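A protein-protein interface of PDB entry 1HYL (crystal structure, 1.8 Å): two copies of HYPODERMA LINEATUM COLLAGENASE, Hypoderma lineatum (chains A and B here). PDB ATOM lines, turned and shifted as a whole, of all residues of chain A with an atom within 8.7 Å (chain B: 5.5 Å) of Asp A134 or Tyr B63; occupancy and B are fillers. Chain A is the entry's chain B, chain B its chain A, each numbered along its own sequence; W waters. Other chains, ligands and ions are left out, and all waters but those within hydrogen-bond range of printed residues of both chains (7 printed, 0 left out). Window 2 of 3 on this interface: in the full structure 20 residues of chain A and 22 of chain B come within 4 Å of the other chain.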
ATOM      1  N   GLU A   6      31.181  -7.958  -7.388  1.00  0.00           N
ATOM      2  CA  GLU A   6      30.444  -6.711  -7.454  1.00  0.00           C
ATOM      3  C   GLU A   6      30.357  -6.235  -8.903  1.00  0.00           C
ATOM      4  O   GLU A   6      31.375  -6.111  -9.591  1.00  0.00           O
ATOM      5  CB  GLU A   6      31.225  -5.705  -6.647  1.00  0.00           C
ATOM      6  CG  GLU A   6      30.391  -4.594  -6.054  1.00  0.00           C
ATOM      7  CD  GLU A   6      31.253  -3.690  -5.195  1.00  0.00           C
ATOM      8  OE1 GLU A   6      31.904  -2.724  -5.740  1.00  0.00           O
ATOM      9  OE2 GLU A   6      31.341  -3.910  -3.932  1.00  0.00           O
ATOM     10  N   ARG A  27       6.172  -5.301   1.406  1.00  0.00           N
ATOM     11  CA  ARG A  27       7.098  -4.885   0.384  1.00  0.00           C
ATOM     12  C   ARG A  27       8.216  -5.940   0.213  1.00  0.00           C
ATOM     13  O   ARG A  27       8.968  -6.291   1.129  1.00  0.00           O
ATOM     14  CB  ARG A  27       7.587  -3.486   0.796  1.00  0.00           C
ATOM     15  CG  ARG A  27       8.620  -3.003  -0.168  1.00  0.00           C
ATOM     16  CD  ARG A  27       8.644  -1.549  -0.408  1.00  0.00           C
ATOM     17  NE  ARG A  27       9.637  -0.904   0.391  1.00  0.00           N
ATOM     18  CZ  ARG A  27      10.484   0.024  -0.076  1.00  0.00           C
ATOM     19  NH1 ARG A  27      10.622   0.360  -1.356  1.00  0.00           N
ATOM     20  NH2 ARG A  27      11.275   0.592   0.828  1.00  0.00           N
ATOM     21  N   VAL A  28       8.285  -6.489  -1.006  1.00  0.00           N
ATOM     22  CA  VAL A  28       9.130  -7.611  -1.409  1.00  0.00           C
ATOM     23  C   VAL A  28      10.149  -7.159  -2.471  1.00  0.00           C
ATOM     24  O   VAL A  28       9.832  -6.250  -3.244  1.00  0.00           O
ATOM     25  CB  VAL A  28       8.170  -8.717  -1.950  1.00  0.00           C
ATOM     26  CG1 VAL A  28       8.892  -9.878  -2.578  1.00  0.00           C
ATOM     27  CG2 VAL A  28       7.431  -9.332  -0.785  1.00  0.00           C
ATOM     28  N   TRP A  29      11.383  -7.695  -2.506  1.00  0.00           N
ATOM     29  CA  TRP A  29      12.341  -7.426  -3.594  1.00  0.00           C
ATOM     30  C   TRP A  29      12.581  -8.703  -4.420  1.00  0.00           C
ATOM     31  O   TRP A  29      12.703  -9.812  -3.884  1.00  0.00           O
ATOM     32  CB  TRP A  29      13.694  -6.990  -3.082  1.00  0.00           C
ATOM     33  CG  TRP A  29      14.627  -6.585  -4.224  1.00  0.00           C
ATOM     34  CD1 TRP A  29      15.548  -7.478  -4.718  1.00  0.00           C
ATOM     35  CD2 TRP A  29      14.650  -5.369  -4.883  1.00  0.00           C
ATOM     36  NE1 TRP A  29      16.151  -6.849  -5.692  1.00  0.00           N
ATOM     37  CE2 TRP A  29      15.663  -5.593  -5.821  1.00  0.00           C
ATOM     38  CE3 TRP A  29      14.015  -4.136  -4.858  1.00  0.00           C
ATOM     39  CZ2 TRP A  29      16.029  -4.599  -6.701  1.00  0.00           C
ATOM     40  CZ3 TRP A  29      14.384  -3.150  -5.745  1.00  0.00           C
ATOM     41  CH2 TRP A  29      15.391  -3.383  -6.660  1.00  0.00           C
ATOM     42  N   GLN A  62      20.796  -0.753  -5.913  1.00  0.00           N
ATOM     43  CA  GLN A  62      19.466  -1.197  -5.565  1.00  0.00           C
ATOM     44  C   GLN A  62      18.523  -0.017  -5.396  1.00  0.00           C
ATOM     45  O   GLN A  62      18.938   0.937  -4.747  1.00  0.00           O
ATOM     46  CB  GLN A  62      19.533  -1.972  -4.285  1.00  0.00           C
ATOM     47  CG  GLN A  62      18.270  -2.792  -4.258  1.00  0.00           C
ATOM     48  CD  GLN A  62      18.135  -3.654  -3.041  1.00  0.00           C
ATOM     49  OE1 GLN A  62      18.955  -3.634  -2.141  1.00  0.00           O
ATOM     50  NE2 GLN A  62      17.115  -4.474  -2.972  1.00  0.00           N
ATOM     51  N   TYR A  63      17.317   0.012  -5.973  1.00  0.00           N
ATOM     52  CA  TYR A  63      16.335   1.111  -5.870  1.00  0.00           C
ATOM     53  C   TYR A  63      16.776   2.407  -6.568  1.00  0.00           C
ATOM     54  O   TYR A  63      16.306   3.504  -6.228  1.00  0.00           O
ATOM     55  CB  TYR A  63      15.966   1.542  -4.422  1.00  0.00           C
ATOM     56  CG  TYR A  63      15.443   0.397  -3.581  1.00  0.00           C
ATOM     57  CD1 TYR A  63      14.139  -0.051  -3.774  1.00  0.00           C
ATOM     58  CD2 TYR A  63      16.272  -0.192  -2.628  1.00  0.00           C
ATOM     59  CE1 TYR A  63      13.653  -1.103  -2.998  1.00  0.00           C
ATOM     60  CE2 TYR A  63      15.789  -1.244  -1.852  1.00  0.00           C
ATOM     61  CZ  TYR A  63      14.479  -1.699  -2.037  1.00  0.00           C
ATOM     62  OH  TYR A  63      14.003  -2.721  -1.283  1.00  0.00           O
ATOM     63  N   TRP A 128      20.339  -8.730  -6.146  1.00  0.00           N
ATOM     64  CA  TRP A 128      20.595  -7.948  -4.951  1.00  0.00           C
ATOM     65  C   TRP A 128      20.134  -8.748  -3.728  1.00  0.00           C
ATOM     66  O   TRP A 128      19.745  -8.224  -2.685  1.00  0.00           O
ATOM     67  CB  TRP A 128      19.838  -6.607  -5.048  1.00  0.00           C
ATOM     68  CG  TRP A 128      20.277  -5.603  -6.113  1.00  0.00           C
ATOM     69  CD1 TRP A 128      21.210  -4.630  -5.818  1.00  0.00           C
ATOM     70  CD2 TRP A 128      19.776  -5.490  -7.397  1.00  0.00           C
ATOM     71  NE1 TRP A 128      21.300  -3.886  -6.909  1.00  0.00           N
ATOM     72  CE2 TRP A 128      20.462  -4.363  -7.862  1.00  0.00           C
ATOM     73  CE3 TRP A 128      18.858  -6.139  -8.215  1.00  0.00           C
ATOM     74  CZ2 TRP A 128      20.243  -3.873  -9.143  1.00  0.00           C
ATOM     75  CZ3 TRP A 128      18.643  -5.644  -9.484  1.00  0.00           C
ATOM     76  CH2 TRP A 128      19.325  -4.526  -9.944  1.00  0.00           C
ATOM     77  N   GLY A 129      20.075 -10.056  -3.816  1.00  0.00           N
ATOM     78  CA  GLY A 129      19.667 -10.893  -2.702  1.00  0.00           C
ATOM     79  C   GLY A 129      20.748 -10.943  -1.615  1.00  0.00           C
ATOM     80  O   GLY A 129      21.823 -10.330  -1.773  1.00  0.00           O
ATOM     81  N   GLN A 130      20.468 -11.710  -0.542  1.00  0.00           N
ATOM     82  CA  GLN A 130      21.343 -11.828   0.629  1.00  0.00           C
ATOM     83  C   GLN A 130      22.717 -12.289   0.196  1.00  0.00           C
ATOM     84  O   GLN A 130      22.891 -13.174  -0.666  1.00  0.00           O
ATOM     85  CB  GLN A 130      20.788 -12.840   1.672  1.00  0.00           C
ATOM     86  CG  GLN A 130      19.688 -12.235   2.567  1.00  0.00           C
ATOM     87  CD  GLN A 130      19.000 -13.141   3.603  1.00  0.00           C
ATOM     88  OE1 GLN A 130      19.332 -14.331   3.735  1.00  0.00           O
ATOM     89  NE2 GLN A 130      18.026 -12.629   4.379  1.00  0.00           N
ATOM     90  N   SER A 131      23.662 -11.506   0.677  1.00  0.00           N
ATOM     91  CA  SER A 131      25.058 -11.794   0.435  1.00  0.00           C
ATOM     92  C   SER A 131      25.758 -11.881   1.790  1.00  0.00           C
ATOM     93  O   SER A 131      25.164 -11.867   2.880  1.00  0.00           O
ATOM     94  CB  SER A 131      25.656 -10.684  -0.454  1.00  0.00           C
ATOM     95  OG  SER A 131      25.519  -9.360   0.022  1.00  0.00           O
ATOM     96  N   ASN A 132      27.069 -12.004   1.757  1.00  0.00           N
ATOM     97  CA  ASN A 132      27.775 -12.056   3.025  1.00  0.00           C
ATOM     98  C   ASN A 132      28.058 -10.660   3.554  1.00  0.00           C
ATOM     99  O   ASN A 132      28.467 -10.484   4.711  1.00  0.00           O
ATOM    100  CB  ASN A 132      29.088 -12.873   2.813  1.00  0.00           C
ATOM    101  CG  ASN A 132      28.826 -14.375   2.673  1.00  0.00           C
ATOM    102  OD1 ASN A 132      27.725 -14.838   2.971  1.00  0.00           O
ATOM    103  ND2 ASN A 132      29.779 -15.176   2.234  1.00  0.00           N
ATOM    104  N   THR A 133      27.822  -9.718   2.691  1.00  0.00           N
ATOM    105  CA  THR A 133      28.014  -8.310   2.991  1.00  0.00           C
ATOM    106  C   THR A 133      26.683  -7.596   2.918  1.00  0.00           C
ATOM    107  O   THR A 133      25.777  -8.006   2.182  1.00  0.00           O
ATOM    108  CB  THR A 133      28.856  -7.660   1.893  1.00  0.00           C
ATOM    109  OG1 THR A 133      28.266  -7.897   0.623  1.00  0.00           O
ATOM    110  CG2 THR A 133      30.288  -8.197   1.839  1.00  0.00           C
ATOM    111  N   ASP A 134      26.582  -6.549   3.681  1.00  0.00           N
ATOM    112  CA  ASP A 134      25.423  -5.679   3.592  1.00  0.00           C
ATOM    113  C   ASP A 134      25.791  -4.643   2.534  1.00  0.00           C
ATOM    114  O   ASP A 134      26.440  -3.632   2.832  1.00  0.00           O
ATOM    115  CB  ASP A 134      25.128  -5.046   4.951  1.00  0.00           C
ATOM    116  CG  ASP A 134      24.252  -5.928   5.852  1.00  0.00           C
ATOM    117  OD1 ASP A 134      23.093  -6.326   5.444  1.00  0.00           O
ATOM    118  OD2 ASP A 134      24.673  -6.275   7.021  1.00  0.00           O
ATOM    119  N   THR A 135      25.394  -4.947   1.310  1.00  0.00           N
ATOM    120  CA  THR A 135      25.705  -4.104   0.146  1.00  0.00           C
ATOM    121  C   THR A 135      24.458  -3.858  -0.700  1.00  0.00           C
ATOM    122  O   THR A 135      23.569  -4.715  -0.792  1.00  0.00           O
ATOM    123  CB  THR A 135      26.758  -4.798  -0.721  1.00  0.00           C
ATOM    124  OG1 THR A 135      27.119  -3.966  -1.812  1.00  0.00           O
ATOM    125  CG2 THR A 135      26.271  -6.128  -1.302  1.00  0.00           C
ATOM    126  N   VAL A 136      24.412  -2.684  -1.305  1.00  0.00           N
ATOM    127  CA  VAL A 136      23.283  -2.306  -2.165  1.00  0.00           C
ATOM    128  C   VAL A 136      23.705  -2.377  -3.650  1.00  0.00           C
ATOM    129  O   VAL A 136      22.952  -1.968  -4.528  1.00  0.00           O
ATOM    130  CB  VAL A 136      22.784  -0.899  -1.826  1.00  0.00           C
ATOM    131  CG1 VAL A 136      22.343  -0.759  -0.366  1.00  0.00           C
ATOM    132  CG2 VAL A 136      23.834   0.185  -2.052  1.00  0.00           C
ATOM    133  N   ILE A 137      24.894  -2.877  -3.988  1.00  0.00           N
ATOM    134  CA  ILE A 137      25.383  -2.979  -5.362  1.00  0.00           C
ATOM    135  C   ILE A 137      25.040  -4.397  -5.772  1.00  0.00           C
ATOM    136  O   ILE A 137      25.166  -5.349  -4.985  1.00  0.00           O
ATOM    137  CB  ILE A 137      26.955  -2.827  -5.496  1.00  0.00           C
ATOM    138  CG1 ILE A 137      27.499  -1.630  -4.729  1.00  0.00           C
ATOM    139  CG2 ILE A 137      27.312  -2.624  -6.963  1.00  0.00           C
ATOM    140  CD1 ILE A 137      26.958  -0.257  -5.141  1.00  0.00           C
ATOM    141  N   GLN A 139      25.206  -7.990  -7.341  1.00  0.00           N
ATOM    142  CA  GLN A 139      26.284  -8.964  -7.236  1.00  0.00           C
ATOM    143  C   GLN A 139      26.044  -9.990  -8.321  1.00  0.00           C
ATOM    144  O   GLN A 139      24.898 -10.103  -8.808  1.00  0.00           O
ATOM    145  CB  GLN A 139      26.261  -9.706  -5.901  1.00  0.00           C
ATOM    146  CG  GLN A 139      26.206  -8.845  -4.654  1.00  0.00           C
ATOM    147  CD  GLN A 139      27.541  -8.203  -4.343  1.00  0.00           C
ATOM    148  OE1 GLN A 139      28.494  -8.932  -4.082  1.00  0.00           O
ATOM    149  NE2 GLN A 139      27.675  -6.876  -4.351  1.00  0.00           N
ATOM    150  N   ASP B  19      14.508  -7.653   8.726  1.00  0.00           N
ATOM    151  CA  ASP B  19      14.697  -8.271   7.433  1.00  0.00           C
ATOM    152  C   ASP B  19      14.139  -9.706   7.582  1.00  0.00           C
ATOM    153  O   ASP B  19      14.745 -10.561   8.242  1.00  0.00           O
ATOM    154  CB  ASP B  19      16.192  -8.251   7.119  1.00  0.00           C
ATOM    155  CG  ASP B  19      16.494  -8.861   5.753  1.00  0.00           C
ATOM    156  OD1 ASP B  19      15.567  -8.929   4.860  1.00  0.00           O
ATOM    157  OD2 ASP B  19      17.670  -9.310   5.494  1.00  0.00           O
ATOM    158  N   ARG B  27      11.921 -12.114   0.583  1.00  0.00           N
ATOM    159  CA  ARG B  27      12.551 -11.217   1.553  1.00  0.00           C
ATOM    160  C   ARG B  27      11.633 -10.027   1.683  1.00  0.00           C
ATOM    161  O   ARG B  27      11.395  -9.330   0.683  1.00  0.00           O
ATOM    162  CB  ARG B  27      13.919 -10.656   1.102  1.00  0.00           C
ATOM    163  CG  ARG B  27      15.097 -11.334   1.718  1.00  0.00           C
ATOM    164  CD  ARG B  27      16.118 -10.312   2.216  1.00  0.00           C
ATOM    165  NE  ARG B  27      16.993  -9.684   1.244  1.00  0.00           N
ATOM    166  CZ  ARG B  27      18.110  -9.020   1.603  1.00  0.00           C
ATOM    167  NH1 ARG B  27      18.392  -8.772   2.882  1.00  0.00           N
ATOM    168  NH2 ARG B  27      18.906  -8.520   0.642  1.00  0.00           N
ATOM    169  N   TRP B  29      10.635  -6.521   4.200  1.00  0.00           N
ATOM    170  CA  TRP B  29      11.151  -5.605   5.196  1.00  0.00           C
ATOM    171  C   TRP B  29       9.954  -5.145   6.045  1.00  0.00           C
ATOM    172  O   TRP B  29       8.884  -4.867   5.484  1.00  0.00           O
ATOM    173  CB  TRP B  29      11.778  -4.368   4.585  1.00  0.00           C
ATOM    174  CG  TRP B  29      12.290  -3.414   5.670  1.00  0.00           C
ATOM    175  CD1 TRP B  29      11.537  -2.363   6.137  1.00  0.00           C
ATOM    176  CD2 TRP B  29      13.501  -3.517   6.314  1.00  0.00           C
ATOM    177  NE1 TRP B  29      12.263  -1.806   7.081  1.00  0.00           N
ATOM    178  CE2 TRP B  29      13.451  -2.457   7.204  1.00  0.00           C
ATOM    179  CE3 TRP B  29      14.617  -4.329   6.271  1.00  0.00           C
ATOM    180  CZ2 TRP B  29      14.533  -2.212   8.047  1.00  0.00           C
ATOM    181  CZ3 TRP B  29      15.695  -4.076   7.121  1.00  0.00           C
ATOM    182  CH2 TRP B  29      15.663  -3.023   8.013  1.00  0.00           C
ATOM    183  N   TYR B  56      17.717  -5.456  13.234  1.00  0.00           N
ATOM    184  CA  TYR B  56      18.707  -4.394  13.238  1.00  0.00           C
ATOM    185  C   TYR B  56      18.309  -3.367  14.289  1.00  0.00           C
ATOM    186  O   TYR B  56      17.149  -2.941  14.300  1.00  0.00           O
ATOM    187  CB  TYR B  56      18.764  -3.731  11.863  1.00  0.00           C
ATOM    188  CG  TYR B  56      19.319  -4.627  10.771  1.00  0.00           C
ATOM    189  CD1 TYR B  56      20.693  -4.658  10.593  1.00  0.00           C
ATOM    190  CD2 TYR B  56      18.501  -5.409   9.980  1.00  0.00           C
ATOM    191  CE1 TYR B  56      21.264  -5.475   9.628  1.00  0.00           C
ATOM    192  CE2 TYR B  56      19.071  -6.220   9.016  1.00  0.00           C
ATOM    193  CZ  TYR B  56      20.447  -6.247   8.845  1.00  0.00           C
ATOM    194  OH  TYR B  56      21.027  -7.014   7.855  1.00  0.00           O
ATOM    195  N   VAL B  61      20.431   3.980   9.593  1.00  0.00           N
ATOM    196  CA  VAL B  61      20.727   3.489   8.251  1.00  0.00           C
ATOM    197  C   VAL B  61      20.132   2.113   8.123  1.00  0.00           C
ATOM    198  O   VAL B  61      20.395   1.264   8.970  1.00  0.00           O
ATOM    199  CB  VAL B  61      22.243   3.396   7.997  1.00  0.00           C
ATOM    200  CG1 VAL B  61      22.454   2.887   6.564  1.00  0.00           C
ATOM    201  CG2 VAL B  61      22.902   4.771   8.200  1.00  0.00           C
ATOM    202  N   GLN B  62      19.346   1.919   7.072  1.00  0.00           N
ATOM    203  CA  GLN B  62      18.736   0.635   6.823  1.00  0.00           C
ATOM    204  C   GLN B  62      19.774  -0.477   6.683  1.00  0.00           C
ATOM    205  O   GLN B  62      20.821  -0.300   6.066  1.00  0.00           O
ATOM    206  CB  GLN B  62      17.919   0.685   5.567  1.00  0.00           C
ATOM    207  CG  GLN B  62      16.909  -0.444   5.523  1.00  0.00           C
ATOM    208  CD  GLN B  62      15.988  -0.376   4.321  1.00  0.00           C
ATOM    209  OE1 GLN B  62      16.087   0.476   3.441  1.00  0.00           O
ATOM    210  NE2 GLN B  62      15.026  -1.255   4.215  1.00  0.00           N
ATOM    211  N   TYR B  63      19.490  -1.658   7.232  1.00  0.00           N
ATOM    212  CA  TYR B  63      20.365  -2.817   7.159  1.00  0.00           C
ATOM    213  C   TYR B  63      21.693  -2.574   7.872  1.00  0.00           C
ATOM    214  O   TYR B  63      22.685  -3.245   7.584  1.00  0.00           O
ATOM    215  CB  TYR B  63      20.683  -3.212   5.726  1.00  0.00           C
ATOM    216  CG  TYR B  63      19.474  -3.691   5.003  1.00  0.00           C
ATOM    217  CD1 TYR B  63      18.915  -4.898   5.360  1.00  0.00           C
ATOM    218  CD2 TYR B  63      18.960  -2.918   3.999  1.00  0.00           C
ATOM    219  CE1 TYR B  63      17.800  -5.345   4.695  1.00  0.00           C
ATOM    220  CE2 TYR B  63      17.846  -3.356   3.322  1.00  0.00           C
ATOM    221  CZ  TYR B  63      17.275  -4.566   3.677  1.00  0.00           C
ATOM    222  OH  TYR B  63      16.137  -5.001   3.008  1.00  0.00           O
ATOM    223  N   GLU B  64      21.750  -1.635   8.808  1.00  0.00           N
ATOM    224  CA  GLU B  64      22.913  -1.430   9.624  1.00  0.00           C
ATOM    225  C   GLU B  64      22.356  -1.365  11.015  1.00  0.00           C
ATOM    226  O   GLU B  64      21.164  -1.133  11.223  1.00  0.00           O
ATOM    227  CB  GLU B  64      23.590  -0.136   9.288  1.00  0.00           C
ATOM    228  CG  GLU B  64      24.546  -0.332   8.104  1.00  0.00           C
ATOM    229  CD  GLU B  64      25.392   0.896   7.755  1.00  0.00           C
ATOM    230  OE1 GLU B  64      25.603   1.748   8.638  1.00  0.00           O
ATOM    231  OE2 GLU B  64      25.834   1.024   6.595  1.00  0.00           O
ATOM    232  N   GLY B  65      23.172  -1.655  12.006  1.00  0.00           N
ATOM    233  CA  GLY B  65      22.734  -1.530  13.370  1.00  0.00           C
ATOM    234  C   GLY B  65      23.940  -1.668  14.254  1.00  0.00           C
ATOM    235  O   GLY B  65      24.975  -2.183  13.810  1.00  0.00           O
HETATM  236  O   HOH W   1      17.111  -8.443  -1.702  1.00  0.00           O
HETATM  237  O   HOH W   2      14.215   0.879   1.012  1.00  0.00           O
HETATM  238  O   HOH W   3       6.458  -5.108   4.233  1.00  0.00           O
HETATM  239  O   HOH W   4      24.925  -4.327   9.232  1.00  0.00           O
HETATM  240  O   HOH W   5      12.907  -2.211   1.905  1.00  0.00           O
HETATM  241  O   HOH W   6      15.966 -12.853   7.094  1.00  0.00           O
HETATM  242  O   HOH W   7      12.188 -11.945  -2.356  1.00  0.00           O
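Arg B27 touches its own counterpart, Arg A27. Arg A27 touches Trp B29, and with the chains exchanged Trp A29 touches Arg B27. 4 positions are printed for both chains. Of the 10 pairs that touch across the chains among the printed residues, 3 have their exchanged pair printed and touching as well.
Among the printed residues, merely in contact across the chains: Arg A27 with Arg B27 (3.9 Å), Arg A27 with Trp B29 (3.5 Å), Val A28 with Arg B27 (3.5 Å), Trp A29 with Arg B27 (3.6 Å), Gly A129 with Arg B27 (3.8 Å), Gln A130 with Asp B19 (3.5 Å), Gln A130 with Arg B27 (3.7 Å) and Asp A134 with Tyr B63 (3.6 Å).
The side-chain carboxylate (OD2) of Asp B19 is in salt-bridge range of the guanidinium group (NH1) of Arg B27 (2.8 Å). The backbone carbonyl oxygen (O) of Val A136 sits close to the indole nitrogen (NE1) of Trp A128, 3.5 Å away.
Of the printed residues of chain B, Val A28 touches Arg B27. Of the printed residues of chain B, Trp A29 touches Arg B27 (3.6 Å). Of the printed residues of chain B, Trp A128 touches Arg B27. Of the printed residues of chain B, Gly A129 touches Arg B27 (3.8 Å). Of the printed residues of chain B, Gln A130 touches Asp B19 (3.5 Å) and Arg B27 (3.7 Å). Asn A132 touches none of the printed residues of chain B. No residue of chain A comes within 4 Å of Gln B62. Of chain A, only Asp A134 (3.6 Å) comes within 4 Å of Tyr B63. The nearest printed residue of chain B that does not touch Asp A134 is Glu B64 (5.7 Å). The nearest printed residue of chain A that does not touch Trp B29 is Val A28 (5.7 Å).
Water W7 lies within hydrogen-bond range of O of Trp A29 (2.7 Å) and N of Arg B27 (3.0 Å). Water W3 bridges the backbone carbonyl oxygen (O) of Trp B29 (2.7 Å) and the backbone NH (N) of Arg A27 (2.8 Å). Water W1 bridges the backbone carbonyl oxygen (O) of Trp A128 (2.8 Å) and the guanidinium group (NH2) of Arg B27 (3.0 Å). Water W4 lies within hydrogen-bond range of the side-chain carboxylate (OD2) of Asp A134 (3.0 Å) and the backbone carbonyl oxygen (O) of Tyr B63 (3.0 Å). Water W2 bridges NH2 of Arg A27 (3.0 Å) and OE1 of Gln B62 (3.1 Å). Water W5 lies within hydrogen-bond range of the side-chain amide nitrogen of Gln B62, the side-chain hydroxyl of Tyr A63 and the guanidinium group of Arg A27.
The side-chain hydroxyl of Tyr B56 is in hydrogen-bond range of the side-chain carboxylate of Asp A134 (3.2 Å). The guanidinium group (NH2) of Arg B27 sits at hydrogen-bond distance from the backbone carbonyl oxygen (O) of Trp A128, at 3.4 Å.
Hydrophobic or aromatic side chains of chain B that line the printed part of chain A: Tyr B56 and Tyr B63. Of the 17 printed residues of chain A, 7 touch a printed residue of chain B. Printed residues of chain A that touch a printed residue of chain B: Arg A27, Val A28, Trp A29, Trp A128, Gly A129, Gln A130 and Asp A134. Among the printed residues, 10 pairs touch across the chains.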
